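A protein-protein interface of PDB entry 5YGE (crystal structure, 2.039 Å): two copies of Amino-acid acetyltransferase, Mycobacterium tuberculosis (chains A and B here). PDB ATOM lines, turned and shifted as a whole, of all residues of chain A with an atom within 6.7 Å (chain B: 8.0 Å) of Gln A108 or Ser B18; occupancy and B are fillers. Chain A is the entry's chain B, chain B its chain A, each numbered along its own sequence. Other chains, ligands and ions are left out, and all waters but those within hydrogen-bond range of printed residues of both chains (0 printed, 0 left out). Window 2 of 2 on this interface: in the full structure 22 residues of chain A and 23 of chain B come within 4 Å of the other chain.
N of Arg B16 is in hydrogen-bond range of OD2 of Asp B19.
O of Ala A104 sits at hydrogen-bond distance from N of Leu A109.
The backbone carbonyl oxygen of Arg A105 sits close to the side-chain amide oxygen of Gln A108 (3.3 Å).
OE1 of Gln A108 lies close to O of Asp A106.
Hydrophobic or aromatic side chains of chain B within 4 Å of the printed part of chain A: Tyr B44.
Of the 12 printed residues of chain A, 5 touch a printed residue of chain B.
Among the printed residues, 9 pairs touch across the chains.
Among the printed residues, no Asp or Glu carboxylate lies within 4 Å of a Lys or Arg side-chain nitrogen of the other chain.
The backbone carbonyl oxygen (O) of Ser A73 is in hydrogen-bond range of the side-chain hydroxyl (OG1) of Thr B17 (3.0 Å).
N of Thr B17 is in hydrogen-bond range of O of Leu A107 (2.9 Å).
The backbone carbonyl oxygen of Gln A108 is in hydrogen-bond range of the side-chain hydroxyl of Thr B17, 3.4 Å away.
Gln A108 touches two residues of chain B.
Ser B18 touches just one residue of chain A: Gln A108 (3.5 Å).
Of the printed residues of chain A, Ala B15 touches Leu A107.
Of the printed residues of chain A, Tyr B44 touches Ser A73.
Printed residues of chain A within 4 Å of Thr B17: Ser A73, Leu A107, Gln A108 and Leu A109.
The nearest residue of chain B that does not touch Gln A108 is Arg B16 (4.02 Å).
The nearest printed residue of chain A that does not touch Tyr B44 is Asp A74 (5.9 Å).
No position is printed for both chains.
Of the 9 pairs that touch across the chains among the printed residues, none has its exchanged pair printed and touching as well.
Among the printed residues, merely in contact across the chains: Ser A73 with Tyr B44 (3.3 Å), Asp A106 with Arg B16 (3.3 Å), Leu A107 with Ala B15 (3.6 Å), Leu A107 with Arg B16 (3.8 Å), Gln A108 with Ser B18 (3.5 Å) and Leu A109 with Thr B17 (3.8 Å).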
ATOM      1  N   SER A  73     -14.093  -1.426  11.048  1.00  0.00           N
ATOM      2  CA  SER A  73     -15.087  -0.621  10.394  1.00  0.00           C
ATOM      3  C   SER A  73     -15.548   0.545  11.255  1.00  0.00           C
ATOM      4  O   SER A  73     -15.907   1.544  10.741  1.00  0.00           O
ATOM      5  CB  SER A  73     -16.296  -1.433   9.970  1.00  0.00           C
ATOM      6  OG  SER A  73     -16.987  -1.887  11.047  1.00  0.00           O
ATOM      7  N   ASP A  74     -15.560   0.402  12.555  1.00  0.00           N
ATOM      8  CA  ASP A  74     -16.121   1.382  13.430  1.00  0.00           C
ATOM      9  C   ASP A  74     -15.131   2.122  14.346  1.00  0.00           C
ATOM     10  O   ASP A  74     -15.524   2.965  15.068  1.00  0.00           O
ATOM     11  CB  ASP A  74     -17.230   0.747  14.260  1.00  0.00           C
ATOM     12  CG  ASP A  74     -16.724  -0.332  15.204  1.00  0.00           C
ATOM     13  OD1 ASP A  74     -15.621  -0.791  15.077  1.00  0.00           O
ATOM     14  OD2 ASP A  74     -17.473  -0.702  16.076  1.00  0.00           O
ATOM     15  N   LEU A  75     -13.866   1.763  14.288  1.00  0.00           N
ATOM     16  CA  LEU A  75     -12.898   2.213  15.243  1.00  0.00           C
ATOM     17  C   LEU A  75     -11.583   2.653  14.656  1.00  0.00           C
ATOM     18  O   LEU A  75     -10.993   1.936  13.868  1.00  0.00           O
ATOM     19  CB  LEU A  75     -12.621   1.136  16.248  1.00  0.00           C
ATOM     20  CG  LEU A  75     -11.550   1.339  17.288  1.00  0.00           C
ATOM     21  CD1 LEU A  75     -12.074   2.381  18.251  1.00  0.00           C
ATOM     22  CD2 LEU A  75     -11.246   0.033  17.991  1.00  0.00           C
ATOM     23  N   VAL A 103     -11.661  13.492   9.457  1.00  0.00           N
ATOM     24  CA  VAL A 103     -11.320  12.370   8.631  1.00  0.00           C
ATOM     25  C   VAL A 103     -12.006  11.095   9.132  1.00  0.00           C
ATOM     26  O   VAL A 103     -12.575  10.374   8.367  1.00  0.00           O
ATOM     27  CB  VAL A 103      -9.805  12.154   8.520  1.00  0.00           C
ATOM     28  CG1 VAL A 103      -9.519  10.888   7.729  1.00  0.00           C
ATOM     29  CG2 VAL A 103      -9.128  13.327   7.836  1.00  0.00           C
ATOM     30  N   ALA A 104     -11.940  10.901  10.436  1.00  0.00           N
ATOM     31  CA  ALA A 104     -12.606   9.811  11.108  1.00  0.00           C
ATOM     32  C   ALA A 104     -14.085   9.784  10.779  1.00  0.00           C
ATOM     33  O   ALA A 104     -14.602   8.802  10.369  1.00  0.00           O
ATOM     34  CB  ALA A 104     -12.367   9.833  12.585  1.00  0.00           C
ATOM     35  N   ARG A 105     -14.713  10.925  10.899  1.00  0.00           N
ATOM     36  CA  ARG A 105     -16.092  11.105  10.464  1.00  0.00           C
ATOM     37  C   ARG A 105     -16.305  10.797   8.952  1.00  0.00           C
ATOM     38  O   ARG A 105     -17.191  10.095   8.584  1.00  0.00           O
ATOM     39  CB  ARG A 105     -16.634  12.493  10.833  1.00  0.00           C
ATOM     40  CG  ARG A 105     -16.975  12.681  12.295  1.00  0.00           C
ATOM     41  CD  ARG A 105     -17.453  14.090  12.633  1.00  0.00           C
ATOM     42  NE  ARG A 105     -16.938  14.459  13.914  1.00  0.00           N
ATOM     43  CZ  ARG A 105     -16.005  15.363  14.117  1.00  0.00           C
ATOM     44  NH1 ARG A 105     -15.527  16.086  13.134  1.00  0.00           N
ATOM     45  NH2 ARG A 105     -15.596  15.568  15.328  1.00  0.00           N
ATOM     46  N   ASP A 106     -15.442  11.321   8.122  1.00  0.00           N
ATOM     47  CA  ASP A 106     -15.578  11.094   6.679  1.00  0.00           C
ATOM     48  C   ASP A 106     -15.471   9.590   6.384  1.00  0.00           C
ATOM     49  O   ASP A 106     -16.163   9.058   5.511  1.00  0.00           O
ATOM     50  CB  ASP A 106     -14.514  11.871   5.901  1.00  0.00           C
ATOM     51  CG  ASP A 106     -14.702  13.383   6.002  1.00  0.00           C
ATOM     52  OD1 ASP A 106     -15.825  13.839   6.323  1.00  0.00           O
ATOM     53  OD2 ASP A 106     -13.716  14.112   5.756  1.00  0.00           O
ATOM     54  N   LEU A 107     -14.613   8.909   7.138  1.00  0.00           N
ATOM     55  CA  LEU A 107     -14.378   7.467   6.918  1.00  0.00           C
ATOM     56  C   LEU A 107     -15.547   6.619   7.424  1.00  0.00           C
ATOM     57  O   LEU A 107     -15.599   5.418   7.169  1.00  0.00           O
ATOM     58  CB  LEU A 107     -13.093   7.024   7.620  1.00  0.00           C
ATOM     59  CG  LEU A 107     -11.808   7.493   6.942  1.00  0.00           C
ATOM     60  CD1 LEU A 107     -10.600   7.193   7.833  1.00  0.00           C
ATOM     61  CD2 LEU A 107     -11.690   6.794   5.590  1.00  0.00           C
ATOM     62  N   GLN A 108     -16.464   7.223   8.147  1.00  0.00           N
ATOM     63  CA  GLN A 108     -17.604   6.561   8.716  1.00  0.00           C
ATOM     64  C   GLN A 108     -17.227   5.697   9.921  1.00  0.00           C
ATOM     65  O   GLN A 108     -17.814   4.708  10.140  1.00  0.00           O
ATOM     66  CB  GLN A 108     -18.371   5.715   7.692  1.00  0.00           C
ATOM     67  CG  GLN A 108     -18.768   6.379   6.420  1.00  0.00           C
ATOM     68  CD  GLN A 108     -19.611   7.598   6.643  1.00  0.00           C
ATOM     69  OE1 GLN A 108     -19.206   8.694   6.354  1.00  0.00           O
ATOM     70  NE2 GLN A 108     -20.788   7.407   7.132  1.00  0.00           N
ATOM     71  N   LEU A 109     -16.213   6.090  10.649  1.00  0.00           N
ATOM     72  CA  LEU A 109     -15.908   5.548  11.932  1.00  0.00           C
ATOM     73  C   LEU A 109     -16.956   5.998  12.991  1.00  0.00           C
ATOM     74  O   LEU A 109     -17.560   7.005  12.845  1.00  0.00           O
ATOM     75  CB  LEU A 109     -14.496   5.937  12.332  1.00  0.00           C
ATOM     76  CG  LEU A 109     -13.303   5.546  11.485  1.00  0.00           C
ATOM     77  CD1 LEU A 109     -12.026   6.018  12.084  1.00  0.00           C
ATOM     78  CD2 LEU A 109     -13.251   4.062  11.273  1.00  0.00           C
ATOM     79  N   GLN A 110     -17.138   5.217  14.029  1.00  0.00           N
ATOM     80  CA  GLN A 110     -18.008   5.581  15.135  1.00  0.00           C
ATOM     81  C   GLN A 110     -17.287   6.032  16.423  1.00  0.00           C
ATOM     82  O   GLN A 110     -17.831   6.790  17.156  1.00  0.00           O
ATOM     83  CB  GLN A 110     -18.968   4.464  15.435  1.00  0.00           C
ATOM     84  CG  GLN A 110     -19.882   4.124  14.278  1.00  0.00           C
ATOM     85  CD  GLN A 110     -20.763   2.913  14.501  1.00  0.00           C
ATOM     86  OE1 GLN A 110     -20.708   2.261  15.507  1.00  0.00           O
ATOM     87  NE2 GLN A 110     -21.578   2.624  13.536  1.00  0.00           N
ATOM     88  N   LEU A 174     -17.903   9.485  18.236  1.00  0.00           N
ATOM     89  CA  LEU A 174     -18.177  10.449  17.215  1.00  0.00           C
ATOM     90  C   LEU A 174     -19.690  10.690  17.133  1.00  0.00           C
ATOM     91  O   LEU A 174     -20.092  11.723  16.671  1.00  0.00           O
ATOM     92  CB  LEU A 174     -17.578  10.047  15.859  1.00  0.00           C
ATOM     93  CG  LEU A 174     -16.076   9.841  15.812  1.00  0.00           C
ATOM     94  CD1 LEU A 174     -15.609   9.304  14.507  1.00  0.00           C
ATOM     95  CD2 LEU A 174     -15.316  11.065  16.196  1.00  0.00           C
ATOM     96  N   ARG B  13     -13.592   8.232  -5.945  1.00  0.00           N
ATOM     97  CA  ARG B  13     -13.465   8.858  -4.662  1.00  0.00           C
ATOM     98  C   ARG B  13     -12.756   7.992  -3.609  1.00  0.00           C
ATOM     99  O   ARG B  13     -12.717   6.823  -3.729  1.00  0.00           O
ATOM    100  CB  ARG B  13     -14.840   9.243  -4.132  1.00  0.00           C
ATOM    101  CG  ARG B  13     -15.673   8.058  -3.734  1.00  0.00           C
ATOM    102  CD  ARG B  13     -16.950   8.418  -2.998  1.00  0.00           C
ATOM    103  NE  ARG B  13     -17.848   7.301  -2.884  1.00  0.00           N
ATOM    104  CZ  ARG B  13     -17.693   6.301  -2.049  1.00  0.00           C
ATOM    105  NH1 ARG B  13     -16.667   6.265  -1.248  1.00  0.00           N
ATOM    106  NH2 ARG B  13     -18.547   5.320  -2.042  1.00  0.00           N
ATOM    107  N   ALA B  15     -12.163   5.777  -0.546  1.00  0.00           N
ATOM    108  CA  ALA B  15     -12.880   4.787   0.207  1.00  0.00           C
ATOM    109  C   ALA B  15     -13.279   5.231   1.616  1.00  0.00           C
ATOM    110  O   ALA B  15     -12.639   6.031   2.228  1.00  0.00           O
ATOM    111  CB  ALA B  15     -12.135   3.488   0.259  1.00  0.00           C
ATOM    112  N   ARG B  16     -14.388   4.695   2.040  1.00  0.00           N
ATOM    113  CA  ARG B  16     -14.865   4.785   3.397  1.00  0.00           C
ATOM    114  C   ARG B  16     -14.961   3.370   3.988  1.00  0.00           C
ATOM    115  O   ARG B  16     -15.017   2.440   3.284  1.00  0.00           O
ATOM    116  CB  ARG B  16     -16.202   5.514   3.445  1.00  0.00           C
ATOM    117  CG  ARG B  16     -16.228   6.732   2.566  1.00  0.00           C
ATOM    118  CD  ARG B  16     -17.329   7.729   2.771  1.00  0.00           C
ATOM    119  NE  ARG B  16     -18.430   7.379   1.947  1.00  0.00           N
ATOM    120  CZ  ARG B  16     -18.977   8.056   0.950  1.00  0.00           C
ATOM    121  NH1 ARG B  16     -18.547   9.225   0.524  1.00  0.00           N
ATOM    122  NH2 ARG B  16     -19.993   7.487   0.369  1.00  0.00           N
ATOM    123  N   THR B  17     -15.007   3.228   5.297  1.00  0.00           N
ATOM    124  CA  THR B  17     -15.180   1.924   5.882  1.00  0.00           C
ATOM    125  C   THR B  17     -16.468   1.265   5.419  1.00  0.00           C
ATOM    126  O   THR B  17     -16.517   0.117   5.283  1.00  0.00           O
ATOM    127  CB  THR B  17     -15.105   1.904   7.421  1.00  0.00           C
ATOM    128  OG1 THR B  17     -16.184   2.614   7.979  1.00  0.00           O
ATOM    129  CG2 THR B  17     -13.737   2.392   7.912  1.00  0.00           C
ATOM    130  N   SER B  18     -17.484   2.059   5.166  1.00  0.00           N
ATOM    131  CA  SER B  18     -18.706   1.558   4.620  1.00  0.00           C
ATOM    132  C   SER B  18     -18.579   0.890   3.256  1.00  0.00           C
ATOM    133  O   SER B  18     -19.432   0.174   2.888  1.00  0.00           O
ATOM    134  CB  SER B  18     -19.777   2.620   4.578  1.00  0.00           C
ATOM    135  OG  SER B  18     -19.286   3.810   4.117  1.00  0.00           O
ATOM    136  N   ASP B  19     -17.529   1.187   2.528  1.00  0.00           N
ATOM    137  CA  ASP B  19     -17.253   0.612   1.233  1.00  0.00           C
ATOM    138  C   ASP B  19     -16.544  -0.737   1.298  1.00  0.00           C
ATOM    139  O   ASP B  19     -16.463  -1.416   0.327  1.00  0.00           O
ATOM    140  CB  ASP B  19     -16.420   1.565   0.419  1.00  0.00           C
ATOM    141  CG  ASP B  19     -17.143   2.835   0.076  1.00  0.00           C
ATOM    142  OD1 ASP B  19     -18.224   2.784  -0.450  1.00  0.00           O
ATOM    143  OD2 ASP B  19     -16.587   3.875   0.334  1.00  0.00           O
ATOM    144  N   VAL B  20     -15.985  -1.073   2.438  1.00  0.00           N
ATOM    145  CA  VAL B  20     -15.147  -2.238   2.542  1.00  0.00           C
ATOM    146  C   VAL B  20     -15.850  -3.558   2.166  1.00  0.00           C
ATOM    147  O   VAL B  20     -15.311  -4.338   1.483  1.00  0.00           O
ATOM    148  CB  VAL B  20     -14.432  -2.285   3.880  1.00  0.00           C
ATOM    149  CG1 VAL B  20     -13.818  -3.631   4.168  1.00  0.00           C
ATOM    150  CG2 VAL B  20     -13.464  -1.148   4.005  1.00  0.00           C
ATOM    151  N   PRO B  21     -17.144  -3.708   2.666  1.00  0.00           N
ATOM    152  CA  PRO B  21     -17.855  -4.903   2.159  1.00  0.00           C
ATOM    153  C   PRO B  21     -17.941  -5.000   0.620  1.00  0.00           C
ATOM    154  O   PRO B  21     -17.707  -6.029   0.098  1.00  0.00           O
ATOM    155  CB  PRO B  21     -19.223  -4.803   2.794  1.00  0.00           C
ATOM    156  CG  PRO B  21     -19.010  -4.092   4.058  1.00  0.00           C
ATOM    157  CD  PRO B  21     -18.129  -3.001   3.628  1.00  0.00           C
ATOM    158  N   ALA B  22     -18.194  -3.908  -0.071  1.00  0.00           N
ATOM    159  CA  ALA B  22     -18.164  -3.896  -1.531  1.00  0.00           C
ATOM    160  C   ALA B  22     -16.793  -4.223  -2.116  1.00  0.00           C
ATOM    161  O   ALA B  22     -16.693  -4.956  -3.033  1.00  0.00           O
ATOM    162  CB  ALA B  22     -18.655  -2.597  -2.065  1.00  0.00           C
ATOM    163  N   ILE B  23     -15.756  -3.655  -1.541  1.00  0.00           N
ATOM    164  CA  ILE B  23     -14.405  -3.950  -1.897  1.00  0.00           C
ATOM    165  C   ILE B  23     -14.087  -5.424  -1.722  1.00  0.00           C
ATOM    166  O   ILE B  23     -13.543  -6.001  -2.586  1.00  0.00           O
ATOM    167  CB  ILE B  23     -13.373  -3.075  -1.159  1.00  0.00           C
ATOM    168  CG1 ILE B  23     -13.497  -1.629  -1.600  1.00  0.00           C
ATOM    169  CG2 ILE B  23     -11.961  -3.546  -1.431  1.00  0.00           C
ATOM    170  CD1 ILE B  23     -12.865  -0.640  -0.680  1.00  0.00           C
ATOM    171  N   TYR B  44      -9.846  -3.038   6.176  1.00  0.00           N
ATOM    172  CA  TYR B  44     -10.157  -1.939   7.066  1.00  0.00           C
ATOM    173  C   TYR B  44      -8.892  -1.117   7.366  1.00  0.00           C
ATOM    174  O   TYR B  44      -8.920   0.016   7.238  1.00  0.00           O
ATOM    175  CB  TYR B  44     -10.879  -2.377   8.340  1.00  0.00           C
ATOM    176  CG  TYR B  44     -12.328  -2.698   8.115  1.00  0.00           C
ATOM    177  CD1 TYR B  44     -13.166  -1.759   7.590  1.00  0.00           C
ATOM    178  CD2 TYR B  44     -12.827  -3.955   8.353  1.00  0.00           C
ATOM    179  CE1 TYR B  44     -14.457  -2.021   7.326  1.00  0.00           C
ATOM    180  CE2 TYR B  44     -14.153  -4.244   8.094  1.00  0.00           C
ATOM    181  CZ  TYR B  44     -14.944  -3.261   7.586  1.00  0.00           C
ATOM    182  OH  TYR B  44     -16.203  -3.482   7.330  1.00  0.00           O
ATOM    183  N   VAL B  47      -7.803   0.971   4.395  1.00  0.00           N
ATOM    184  CA  VAL B  47      -8.875   1.703   3.788  1.00  0.00           C
ATOM    185  C   VAL B  47      -8.440   3.058   3.192  1.00  0.00           C
ATOM    186  O   VAL B  47      -8.872   3.434   2.150  1.00  0.00           O
ATOM    187  CB  VAL B  47     -10.090   1.853   4.712  1.00  0.00           C
ATOM    188  CG1 VAL B  47      -9.825   2.794   5.864  1.00  0.00           C
ATOM    189  CG2 VAL B  47     -11.312   2.186   3.906  1.00  0.00           C
ATOM    190  N   VAL B  62     -20.880   1.263  -5.656  1.00  0.00           N
ATOM    191  CA  VAL B  62     -19.482   0.976  -5.908  1.00  0.00           C
ATOM    192  C   VAL B  62     -19.350  -0.142  -6.956  1.00  0.00           C
ATOM    193  O   VAL B  62     -19.808  -1.209  -6.751  1.00  0.00           O
ATOM    194  CB  VAL B  62     -18.721   0.665  -4.610  1.00  0.00           C
ATOM    195  CG1 VAL B  62     -17.403  -0.025  -4.865  1.00  0.00           C
ATOM    196  CG2 VAL B  62     -18.563   1.909  -3.762  1.00  0.00           C
